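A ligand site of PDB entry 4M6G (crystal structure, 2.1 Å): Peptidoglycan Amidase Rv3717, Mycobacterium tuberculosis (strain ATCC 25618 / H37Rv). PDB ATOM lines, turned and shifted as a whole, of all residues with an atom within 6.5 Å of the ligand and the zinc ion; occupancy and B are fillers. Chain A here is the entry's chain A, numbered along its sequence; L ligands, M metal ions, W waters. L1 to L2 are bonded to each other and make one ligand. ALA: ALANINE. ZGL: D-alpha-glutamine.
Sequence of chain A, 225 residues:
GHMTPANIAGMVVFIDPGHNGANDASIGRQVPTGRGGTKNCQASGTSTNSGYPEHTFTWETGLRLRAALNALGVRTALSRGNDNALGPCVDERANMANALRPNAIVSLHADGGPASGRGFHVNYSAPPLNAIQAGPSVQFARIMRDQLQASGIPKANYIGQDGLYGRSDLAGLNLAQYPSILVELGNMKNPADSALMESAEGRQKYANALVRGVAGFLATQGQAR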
ATOM      1  N   GLY A  18     -14.227  23.572  17.512  1.00  0.00           N
ATOM      2  CA  GLY A  18     -14.466  23.654  16.076  1.00  0.00           C
ATOM      3  C   GLY A  18     -14.978  22.379  15.440  1.00  0.00           C
ATOM      4  O   GLY A  18     -14.635  21.280  15.876  1.00  0.00           O
ATOM      5  N   HIS A  19     -15.830  22.553  14.430  1.00  0.00           N
ATOM      6  CA  HIS A  19     -16.398  21.464  13.628  1.00  0.00           C
ATOM      7  C   HIS A  19     -17.428  20.580  14.352  1.00  0.00           C
ATOM      8  O   HIS A  19     -17.720  20.794  15.523  1.00  0.00           O
ATOM      9  CB  HIS A  19     -15.288  20.601  12.999  1.00  0.00           C
ATOM     10  CG  HIS A  19     -14.262  21.388  12.249  1.00  0.00           C
ATOM     11  ND1 HIS A  19     -14.417  21.750  10.916  1.00  0.00           N
ATOM     12  CD2 HIS A  19     -13.058  21.877  12.628  1.00  0.00           C
ATOM     13  CE1 HIS A  19     -13.362  22.428  10.530  1.00  0.00           C
ATOM     14  NE2 HIS A  19     -12.509  22.519  11.545  1.00  0.00           N
ATOM     15  N   THR A  33     -21.233  35.422   6.163  1.00  0.00           N
ATOM     16  CA  THR A  33     -19.842  35.510   6.608  1.00  0.00           C
ATOM     17  C   THR A  33     -19.701  36.588   7.669  1.00  0.00           C
ATOM     18  O   THR A  33     -18.747  36.600   8.437  1.00  0.00           O
ATOM     19  CB  THR A  33     -18.893  35.863   5.449  1.00  0.00           C
ATOM     20  OG1 THR A  33     -19.216  37.172   4.951  1.00  0.00           O
ATOM     21  CG2 THR A  33     -18.992  34.849   4.332  1.00  0.00           C
ATOM     22  N   LYS A  39     -20.648  31.642   3.115  1.00  0.00           N
ATOM     23  CA  LYS A  39     -19.701  30.529   3.068  1.00  0.00           C
ATOM     24  C   LYS A  39     -20.440  29.283   3.550  1.00  0.00           C
ATOM     25  O   LYS A  39     -21.584  29.373   3.993  1.00  0.00           O
ATOM     26  CB  LYS A  39     -18.489  30.810   3.963  1.00  0.00           C
ATOM     27  CG  LYS A  39     -18.758  30.700   5.454  1.00  0.00           C
ATOM     28  CD  LYS A  39     -17.577  31.197   6.265  1.00  0.00           C
ATOM     29  CE  LYS A  39     -16.287  30.522   5.848  1.00  0.00           C
ATOM     30  NZ  LYS A  39     -15.097  31.107   6.523  1.00  0.00           N
ATOM     31  N   ASN A  40     -19.781  28.137   3.453  1.00  0.00           N
ATOM     32  CA  ASN A  40     -20.396  26.880   3.866  1.00  0.00           C
ATOM     33  C   ASN A  40     -20.723  26.859   5.349  1.00  0.00           C
ATOM     34  O   ASN A  40     -19.956  27.363   6.177  1.00  0.00           O
ATOM     35  CB  ASN A  40     -19.490  25.692   3.499  1.00  0.00           C
ATOM     36  CG  ASN A  40     -19.497  25.409   2.012  1.00  0.00           C
ATOM     37  OD1 ASN A  40     -20.009  26.191   1.213  1.00  0.00           O
ATOM     38  ND2 ASN A  40     -18.928  24.277   1.629  1.00  0.00           N
ATOM     39  N   CYS A  41     -21.874  26.277   5.682  1.00  0.00           N
ATOM     40  CA  CYS A  41     -22.350  26.156   7.059  1.00  0.00           C
ATOM     41  C   CYS A  41     -21.279  25.565   7.974  1.00  0.00           C
ATOM     42  O   CYS A  41     -21.028  26.076   9.067  1.00  0.00           O
ATOM     43  CB  CYS A  41     -23.610  25.301   7.118  1.00  0.00           C
ATOM     44  SG  CYS A  41     -23.921  24.495   8.707  1.00  0.00           S
ATOM     45  N   GLN A  42     -20.648  24.496   7.501  1.00  0.00           N
ATOM     46  CA  GLN A  42     -19.545  23.888   8.241  1.00  0.00           C
ATOM     47  C   GLN A  42     -18.492  23.302   7.309  1.00  0.00           C
ATOM     48  O   GLN A  42     -18.618  23.335   6.098  1.00  0.00           O
ATOM     49  CB  GLN A  42     -20.071  22.791   9.173  1.00  0.00           C
ATOM     50  CG  GLN A  42     -20.352  23.260  10.590  1.00  0.00           C
ATOM     51  CD  GLN A  42     -19.108  23.746  11.318  1.00  0.00           C
ATOM     52  OE1 GLN A  42     -17.982  23.417  10.939  1.00  0.00           O
ATOM     53  NE2 GLN A  42     -19.308  24.536  12.359  1.00  0.00           N
ATOM     54  N   ALA A  43     -17.436  22.770   7.928  1.00  0.00           N
ATOM     55  CA  ALA A  43     -16.401  22.040   7.229  1.00  0.00           C
ATOM     56  C   ALA A  43     -16.016  20.849   8.100  1.00  0.00           C
ATOM     57  O   ALA A  43     -16.087  20.933   9.327  1.00  0.00           O
ATOM     58  CB  ALA A  43     -15.199  22.923   6.969  1.00  0.00           C
ATOM     59  N   SER A  44     -15.616  19.751   7.464  1.00  0.00           N
ATOM     60  CA  SER A  44     -15.341  18.522   8.209  1.00  0.00           C
ATOM     61  C   SER A  44     -14.077  18.615   9.057  1.00  0.00           C
ATOM     62  O   SER A  44     -13.944  17.913  10.059  1.00  0.00           O
ATOM     63  CB  SER A  44     -15.250  17.321   7.253  1.00  0.00           C
ATOM     64  OG  SER A  44     -14.179  17.469   6.341  1.00  0.00           O
ATOM     65  N   GLY A  45     -13.165  19.489   8.674  1.00  0.00           N
ATOM     66  CA  GLY A  45     -11.917  19.656   9.395  1.00  0.00           C
ATOM     67  C   GLY A  45     -10.864  18.650   8.977  1.00  0.00           C
ATOM     68  O   GLY A  45     -11.139  17.725   8.213  1.00  0.00           O
ATOM     69  N   THR A  46      -9.649  18.823   9.483  1.00  0.00           N
ATOM     70  CA  THR A  46      -8.526  17.964   9.110  1.00  0.00           C
ATOM     71  C   THR A  46      -8.300  16.853  10.121  1.00  0.00           C
ATOM     72  O   THR A  46      -9.137  16.605  10.987  1.00  0.00           O
ATOM     73  CB  THR A  46      -7.240  18.786   8.927  1.00  0.00           C
ATOM     74  OG1 THR A  46      -6.169  17.924   8.524  1.00  0.00           O
ATOM     75  CG2 THR A  46      -6.862  19.480  10.238  1.00  0.00           C
ATOM     76  N   GLU A  54      -9.571  16.426  13.691  1.00  0.00           N
ATOM     77  CA  GLU A  54      -9.590  17.769  14.308  1.00  0.00           C
ATOM     78  C   GLU A  54     -10.780  17.900  15.244  1.00  0.00           C
ATOM     79  O   GLU A  54     -10.657  18.441  16.353  1.00  0.00           O
ATOM     80  CB  GLU A  54      -9.629  18.912  13.253  1.00  0.00           C
ATOM     81  CG  GLU A  54      -9.466  20.349  13.863  1.00  0.00           C
ATOM     82  CD  GLU A  54      -9.854  21.560  12.955  1.00  0.00           C
ATOM     83  OE1 GLU A  54      -9.755  22.681  13.451  1.00  0.00           O
ATOM     84  OE2 GLU A  54     -10.222  21.435  11.777  1.00  0.00           O
ATOM     85  N   THR A  58     -10.508  19.023  19.178  1.00  0.00           N
ATOM     86  CA  THR A  58     -11.088  20.244  19.708  1.00  0.00           C
ATOM     87  C   THR A  58     -12.154  19.944  20.762  1.00  0.00           C
ATOM     88  O   THR A  58     -12.277  20.663  21.754  1.00  0.00           O
ATOM     89  CB  THR A  58     -11.674  21.130  18.594  1.00  0.00           C
ATOM     90  OG1 THR A  58     -12.720  20.430  17.916  1.00  0.00           O
ATOM     91  CG2 THR A  58     -10.590  21.503  17.590  1.00  0.00           C
ATOM     92  N   VAL A  90     -21.441  27.852  11.345  1.00  0.00           N
ATOM     93  CA  VAL A  90     -20.446  28.762  11.890  1.00  0.00           C
ATOM     94  C   VAL A  90     -21.014  30.123  12.287  1.00  0.00           C
ATOM     95  O   VAL A  90     -20.489  30.775  13.185  1.00  0.00           O
ATOM     96  CB  VAL A  90     -19.243  28.934  10.927  1.00  0.00           C
ATOM     97  CG1 VAL A  90     -18.582  27.591  10.685  1.00  0.00           C
ATOM     98  CG2 VAL A  90     -19.698  29.561   9.624  1.00  0.00           C
ATOM     99  N   LEU A 108     -11.638  26.757  19.215  1.00  0.00           N
ATOM    100  CA  LEU A 108     -10.483  25.860  19.108  1.00  0.00           C
ATOM    101  C   LEU A 108     -10.441  25.141  17.767  1.00  0.00           C
ATOM    102  O   LEU A 108     -11.444  24.582  17.319  1.00  0.00           O
ATOM    103  CB  LEU A 108     -10.482  24.854  20.250  1.00  0.00           C
ATOM    104  CG  LEU A 108     -10.665  25.413  21.660  1.00  0.00           C
ATOM    105  CD1 LEU A 108     -10.485  24.325  22.704  1.00  0.00           C
ATOM    106  CD2 LEU A 108      -9.701  26.549  21.921  1.00  0.00           C
ATOM    107  N   HIS A 109      -9.273  25.154  17.138  1.00  0.00           N
ATOM    108  CA  HIS A 109      -9.048  24.464  15.882  1.00  0.00           C
ATOM    109  C   HIS A 109      -7.638  23.891  15.825  1.00  0.00           C
ATOM    110  O   HIS A 109      -6.793  24.226  16.655  1.00  0.00           O
ATOM    111  CB  HIS A 109      -9.245  25.434  14.699  1.00  0.00           C
ATOM    112  CG  HIS A 109     -10.673  25.675  14.352  1.00  0.00           C
ATOM    113  ND1 HIS A 109     -11.319  25.022  13.318  1.00  0.00           N
ATOM    114  CD2 HIS A 109     -11.587  26.518  14.885  1.00  0.00           C
ATOM    115  CE1 HIS A 109     -12.562  25.434  13.249  1.00  0.00           C
ATOM    116  NE2 HIS A 109     -12.755  26.346  14.194  1.00  0.00           N
ATOM    117  N   ALA A 110      -7.407  23.004  14.871  1.00  0.00           N
ATOM    118  CA  ALA A 110      -6.054  22.530  14.578  1.00  0.00           C
ATOM    119  C   ALA A 110      -5.844  22.500  13.063  1.00  0.00           C
ATOM    120  O   ALA A 110      -6.751  22.138  12.314  1.00  0.00           O
ATOM    121  CB  ALA A 110      -5.811  21.173  15.200  1.00  0.00           C
ATOM    122  N   ASP A 111      -4.648  22.898  12.634  1.00  0.00           N
ATOM    123  CA  ASP A 111      -4.393  23.152  11.214  1.00  0.00           C
ATOM    124  C   ASP A 111      -4.035  21.884  10.444  1.00  0.00           C
ATOM    125  O   ASP A 111      -3.710  20.856  11.037  1.00  0.00           O
ATOM    126  CB  ASP A 111      -3.277  24.190  11.095  1.00  0.00           C
ATOM    127  CG  ASP A 111      -3.181  24.808   9.706  1.00  0.00           C
ATOM    128  OD1 ASP A 111      -4.154  24.690   8.926  1.00  0.00           O
ATOM    129  OD2 ASP A 111      -2.137  25.422   9.397  1.00  0.00           O
ATOM    130  N   GLY A 112      -4.110  21.974   9.122  1.00  0.00           N
ATOM    131  CA  GLY A 112      -3.639  20.916   8.249  1.00  0.00           C
ATOM    132  C   GLY A 112      -2.689  21.510   7.231  1.00  0.00           C
ATOM    133  O   GLY A 112      -3.004  21.612   6.041  1.00  0.00           O
ATOM    134  N   ARG A 167      -7.678  38.172  10.519  1.00  0.00           N
ATOM    135  CA  ARG A 167      -8.503  37.514   9.527  1.00  0.00           C
ATOM    136  C   ARG A 167      -9.762  38.322   9.208  1.00  0.00           C
ATOM    137  O   ARG A 167     -10.323  38.985  10.081  1.00  0.00           O
ATOM    138  CB  ARG A 167      -8.901  36.112   9.998  1.00  0.00           C
ATOM    139  CG  ARG A 167      -7.739  35.230  10.414  1.00  0.00           C
ATOM    140  CD  ARG A 167      -6.919  34.781   9.205  1.00  0.00           C
ATOM    141  NE  ARG A 167      -7.683  33.910   8.319  1.00  0.00           N
ATOM    142  CZ  ARG A 167      -7.703  32.588   8.402  1.00  0.00           C
ATOM    143  NH1 ARG A 167      -6.994  31.967   9.331  1.00  0.00           N
ATOM    144  NH2 ARG A 167      -8.421  31.882   7.543  1.00  0.00           N
ATOM    145  N   ASP A 169     -11.989  36.554   7.011  1.00  0.00           N
ATOM    146  CA  ASP A 169     -12.753  35.491   6.376  1.00  0.00           C
ATOM    147  C   ASP A 169     -13.476  34.548   7.342  1.00  0.00           C
ATOM    148  O   ASP A 169     -14.185  33.634   6.907  1.00  0.00           O
ATOM    149  CB  ASP A 169     -11.858  34.678   5.456  1.00  0.00           C
ATOM    150  CG  ASP A 169     -10.638  34.115   6.172  1.00  0.00           C
ATOM    151  OD1 ASP A 169     -10.118  34.785   7.081  1.00  0.00           O
ATOM    152  OD2 ASP A 169     -10.211  32.997   5.815  1.00  0.00           O
ATOM    153  N   LEU A 170     -13.307  34.754   8.638  1.00  0.00           N
ATOM    154  CA  LEU A 170     -13.894  33.856   9.623  1.00  0.00           C
ATOM    155  C   LEU A 170     -15.208  34.387  10.181  1.00  0.00           C
ATOM    156  O   LEU A 170     -15.236  35.414  10.869  1.00  0.00           O
ATOM    157  CB  LEU A 170     -12.891  33.568  10.751  1.00  0.00           C
ATOM    158  CG  LEU A 170     -11.554  33.014  10.260  1.00  0.00           C
ATOM    159  CD1 LEU A 170     -10.588  32.820  11.415  1.00  0.00           C
ATOM    160  CD2 LEU A 170     -11.758  31.707   9.495  1.00  0.00           C
ATOM    161  N   ALA A 171     -16.288  33.685   9.872  1.00  0.00           N
ATOM    162  CA  ALA A 171     -17.628  34.106  10.269  1.00  0.00           C
ATOM    163  C   ALA A 171     -17.778  34.200  11.786  1.00  0.00           C
ATOM    164  O   ALA A 171     -18.398  35.128  12.293  1.00  0.00           O
ATOM    165  CB  ALA A 171     -18.672  33.163   9.684  1.00  0.00           C
ATOM    166  N   GLY A 172     -17.213  33.225  12.497  1.00  0.00           N
ATOM    167  CA  GLY A 172     -17.255  33.216  13.945  1.00  0.00           C
ATOM    168  C   GLY A 172     -16.645  34.468  14.548  1.00  0.00           C
ATOM    169  O   GLY A 172     -17.121  34.972  15.563  1.00  0.00           O
ATOM    170  N   LEU A 173     -15.587  34.976  13.909  1.00  0.00           N
ATOM    171  CA  LEU A 173     -14.922  36.185  14.374  1.00  0.00           C
ATOM    172  C   LEU A 173     -15.611  37.450  13.877  1.00  0.00           C
ATOM    173  O   LEU A 173     -15.773  38.409  14.620  1.00  0.00           O
ATOM    174  CB  LEU A 173     -13.454  36.183  13.954  1.00  0.00           C
ATOM    175  CG  LEU A 173     -12.542  35.184  14.670  1.00  0.00           C
ATOM    176  CD1 LEU A 173     -11.113  35.288  14.155  1.00  0.00           C
ATOM    177  CD2 LEU A 173     -12.593  35.411  16.176  1.00  0.00           C
ATOM    178  N   LEU A 182      -9.952  33.011  17.758  1.00  0.00           N
ATOM    179  CA  LEU A 182      -9.928  31.629  17.294  1.00  0.00           C
ATOM    180  C   LEU A 182      -8.492  31.119  17.296  1.00  0.00           C
ATOM    181  O   LEU A 182      -7.641  31.618  16.556  1.00  0.00           O
ATOM    182  CB  LEU A 182     -10.547  31.512  15.900  1.00  0.00           C
ATOM    183  CG  LEU A 182     -10.741  30.115  15.314  1.00  0.00           C
ATOM    184  CD1 LEU A 182     -12.008  30.053  14.477  1.00  0.00           C
ATOM    185  CD2 LEU A 182      -9.542  29.694  14.475  1.00  0.00           C
ATOM    186  N   GLU A 184      -5.730  28.382  16.517  1.00  0.00           N
ATOM    187  CA  GLU A 184      -5.223  27.179  15.863  1.00  0.00           C
ATOM    188  C   GLU A 184      -4.075  26.671  16.722  1.00  0.00           C
ATOM    189  O   GLU A 184      -3.028  27.304  16.809  1.00  0.00           O
ATOM    190  CB  GLU A 184      -4.743  27.494  14.448  1.00  0.00           C
ATOM    191  CG  GLU A 184      -5.842  27.905  13.485  1.00  0.00           C
ATOM    192  CD  GLU A 184      -6.477  26.704  12.799  1.00  0.00           C
ATOM    193  OE1 GLU A 184      -7.277  26.922  11.863  1.00  0.00           O
ATOM    194  OE2 GLU A 184      -6.176  25.562  13.189  1.00  0.00           O
HETATM  195  N   ALA L   1     -10.210  23.956   9.868  1.00  0.00           N
HETATM  196  CA  ALA L   1     -10.575  25.314   9.791  1.00  0.00           C
HETATM  197  C   ALA L   1     -11.963  25.458   9.311  1.00  0.00           C
HETATM  198  O   ALA L   1     -12.467  24.577   8.655  1.00  0.00           O
HETATM  199  CB  ALA L   1      -9.629  26.015   8.807  1.00  0.00           C
HETATM  200  CD  ZGL L   2     -15.009  25.986  10.045  1.00  0.00           C
HETATM  201  N   ZGL L   2     -12.695  26.629   9.618  1.00  0.00           N
HETATM  202  O2  ZGL L   2     -14.702  25.706  11.210  1.00  0.00           O
HETATM  203  N1  ZGL L   2     -16.276  25.552   9.512  1.00  0.00           N
HETATM  204  CA  ZGL L   2     -14.054  26.766   9.153  1.00  0.00           C
HETATM  205  CB  ZGL L   2     -14.445  28.222   9.111  1.00  0.00           C
HETATM  206  C   ZGL L   2     -15.632  30.276  10.207  1.00  0.00           C
HETATM  207  CG  ZGL L   2     -15.305  28.777  10.224  1.00  0.00           C
HETATM  208  OXT ZGL L   2     -15.589  30.935  11.298  1.00  0.00           O
HETATM  209  O   ZGL L   2     -15.933  30.849   9.123  1.00  0.00           O
HETATM  210 ZN    ZN M   1     -10.813  23.510  11.997  1.00  0.00          ZN
HETATM  211  O   HOH W   1     -15.407  29.950  13.696  1.00  0.00           O
HETATM  212  O   HOH W   2     -17.390  26.424   6.690  1.00  0.00           O
HETATM  213  O   HOH W   3     -16.472  25.260  13.456  1.00  0.00           O
HETATM  214  O   HOH W   4      -7.668  24.438  10.863  1.00  0.00           O
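Water W4 lies within hydrogen-bond range of OE1 of Glu 184 and O of Ala 110.
Water W3 lies within hydrogen-bond range of O2 of ZGL L2 (2.9 Å), N of His 19 (2.9 Å) and NE2 of Gln 42 (3.1 Å).
Water W2 lies within hydrogen-bond range of the backbone carbonyl oxygen of Asn 40 (2.8 Å), a nitrogen (N1) of ZGL L2 (3.2 Å) and the backbone carbonyl oxygen of Gln 42 (3.4 Å).
A nitrogen (N1) of ZGL L2 lies close to the backbone NH (N) of Ala 43, at 3.4 Å.
Merely in contact with the ligand: Val 90, Leu 170, Glu 184 and Asp 169.
Hydrophobic or aromatic side chains that line the ligand: His 19, Ala 43, Val 90, His 109, Leu 170 and Ala 171.
12 residues have an atom within 4 Å of the ligand: His 19, Lys 39, Gln 42, Ala 43, Glu 54, Val 90, His 109, Asp 169, Leu 170, Ala 171, Gly 172 and Glu 184.
The nearest printed residue that does not touch the ligand is Ala 110 (4.6 Å).
The zinc ion is bound by OE1 of Glu 54, NE2 of His 19, ND1 of His 109, OE2 of Glu 54 and N of ALA L1.
The zinc ion has five donor atoms within binding distance.
Three residues have an atom within 4 Å of the zinc ion: His 19, Glu 54 and His 109.
The side-chain amino group (NZ) of Lys 39 is in salt-bridge range of an oxygen (O) of ZGL L2 (2.7 Å).
N of Gly 172 lies within hydrogen-bond range of OXT of ZGL L2, at 3.1 Å.
OE1 of Gln 42 sits at hydrogen-bond distance from N1 of ZGL L2, at 3.1 Å.
N of Ala 171 sits at hydrogen-bond distance from O of ZGL L2 (3.0 Å).
OE1 of Glu 54 lies close to N of Ala 110.
The backbone NH (N) of Asp 111 sits at hydrogen-bond distance from the side-chain carboxylate (OE2) of Glu 184, at 3.1 Å.
ND1 of His 19 sits at hydrogen-bond distance from N of Gly 45 (3.4 Å).
The backbone NH (N) of Glu 54 lies within hydrogen-bond range of the backbone carbonyl oxygen (O) of Thr 46, 2.7 Å away.
ND1 of His 19 is in hydrogen-bond range of O of Ala 43 (2.4 Å).
The side-chain carboxylate (OD2) of Asp 169 lies within salt-bridge range of the guanidinium group (NH2) of Arg 167, 2.7 Å away.
The side-chain carboxylate (OE2) of Glu 184 sits close to the backbone NH (N) of Ala 110, at 3.3 Å.
The backbone NH (N) of Val 90 is in hydrogen-bond range of the backbone carbonyl oxygen (O) of Cys 41 (2.9 Å).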
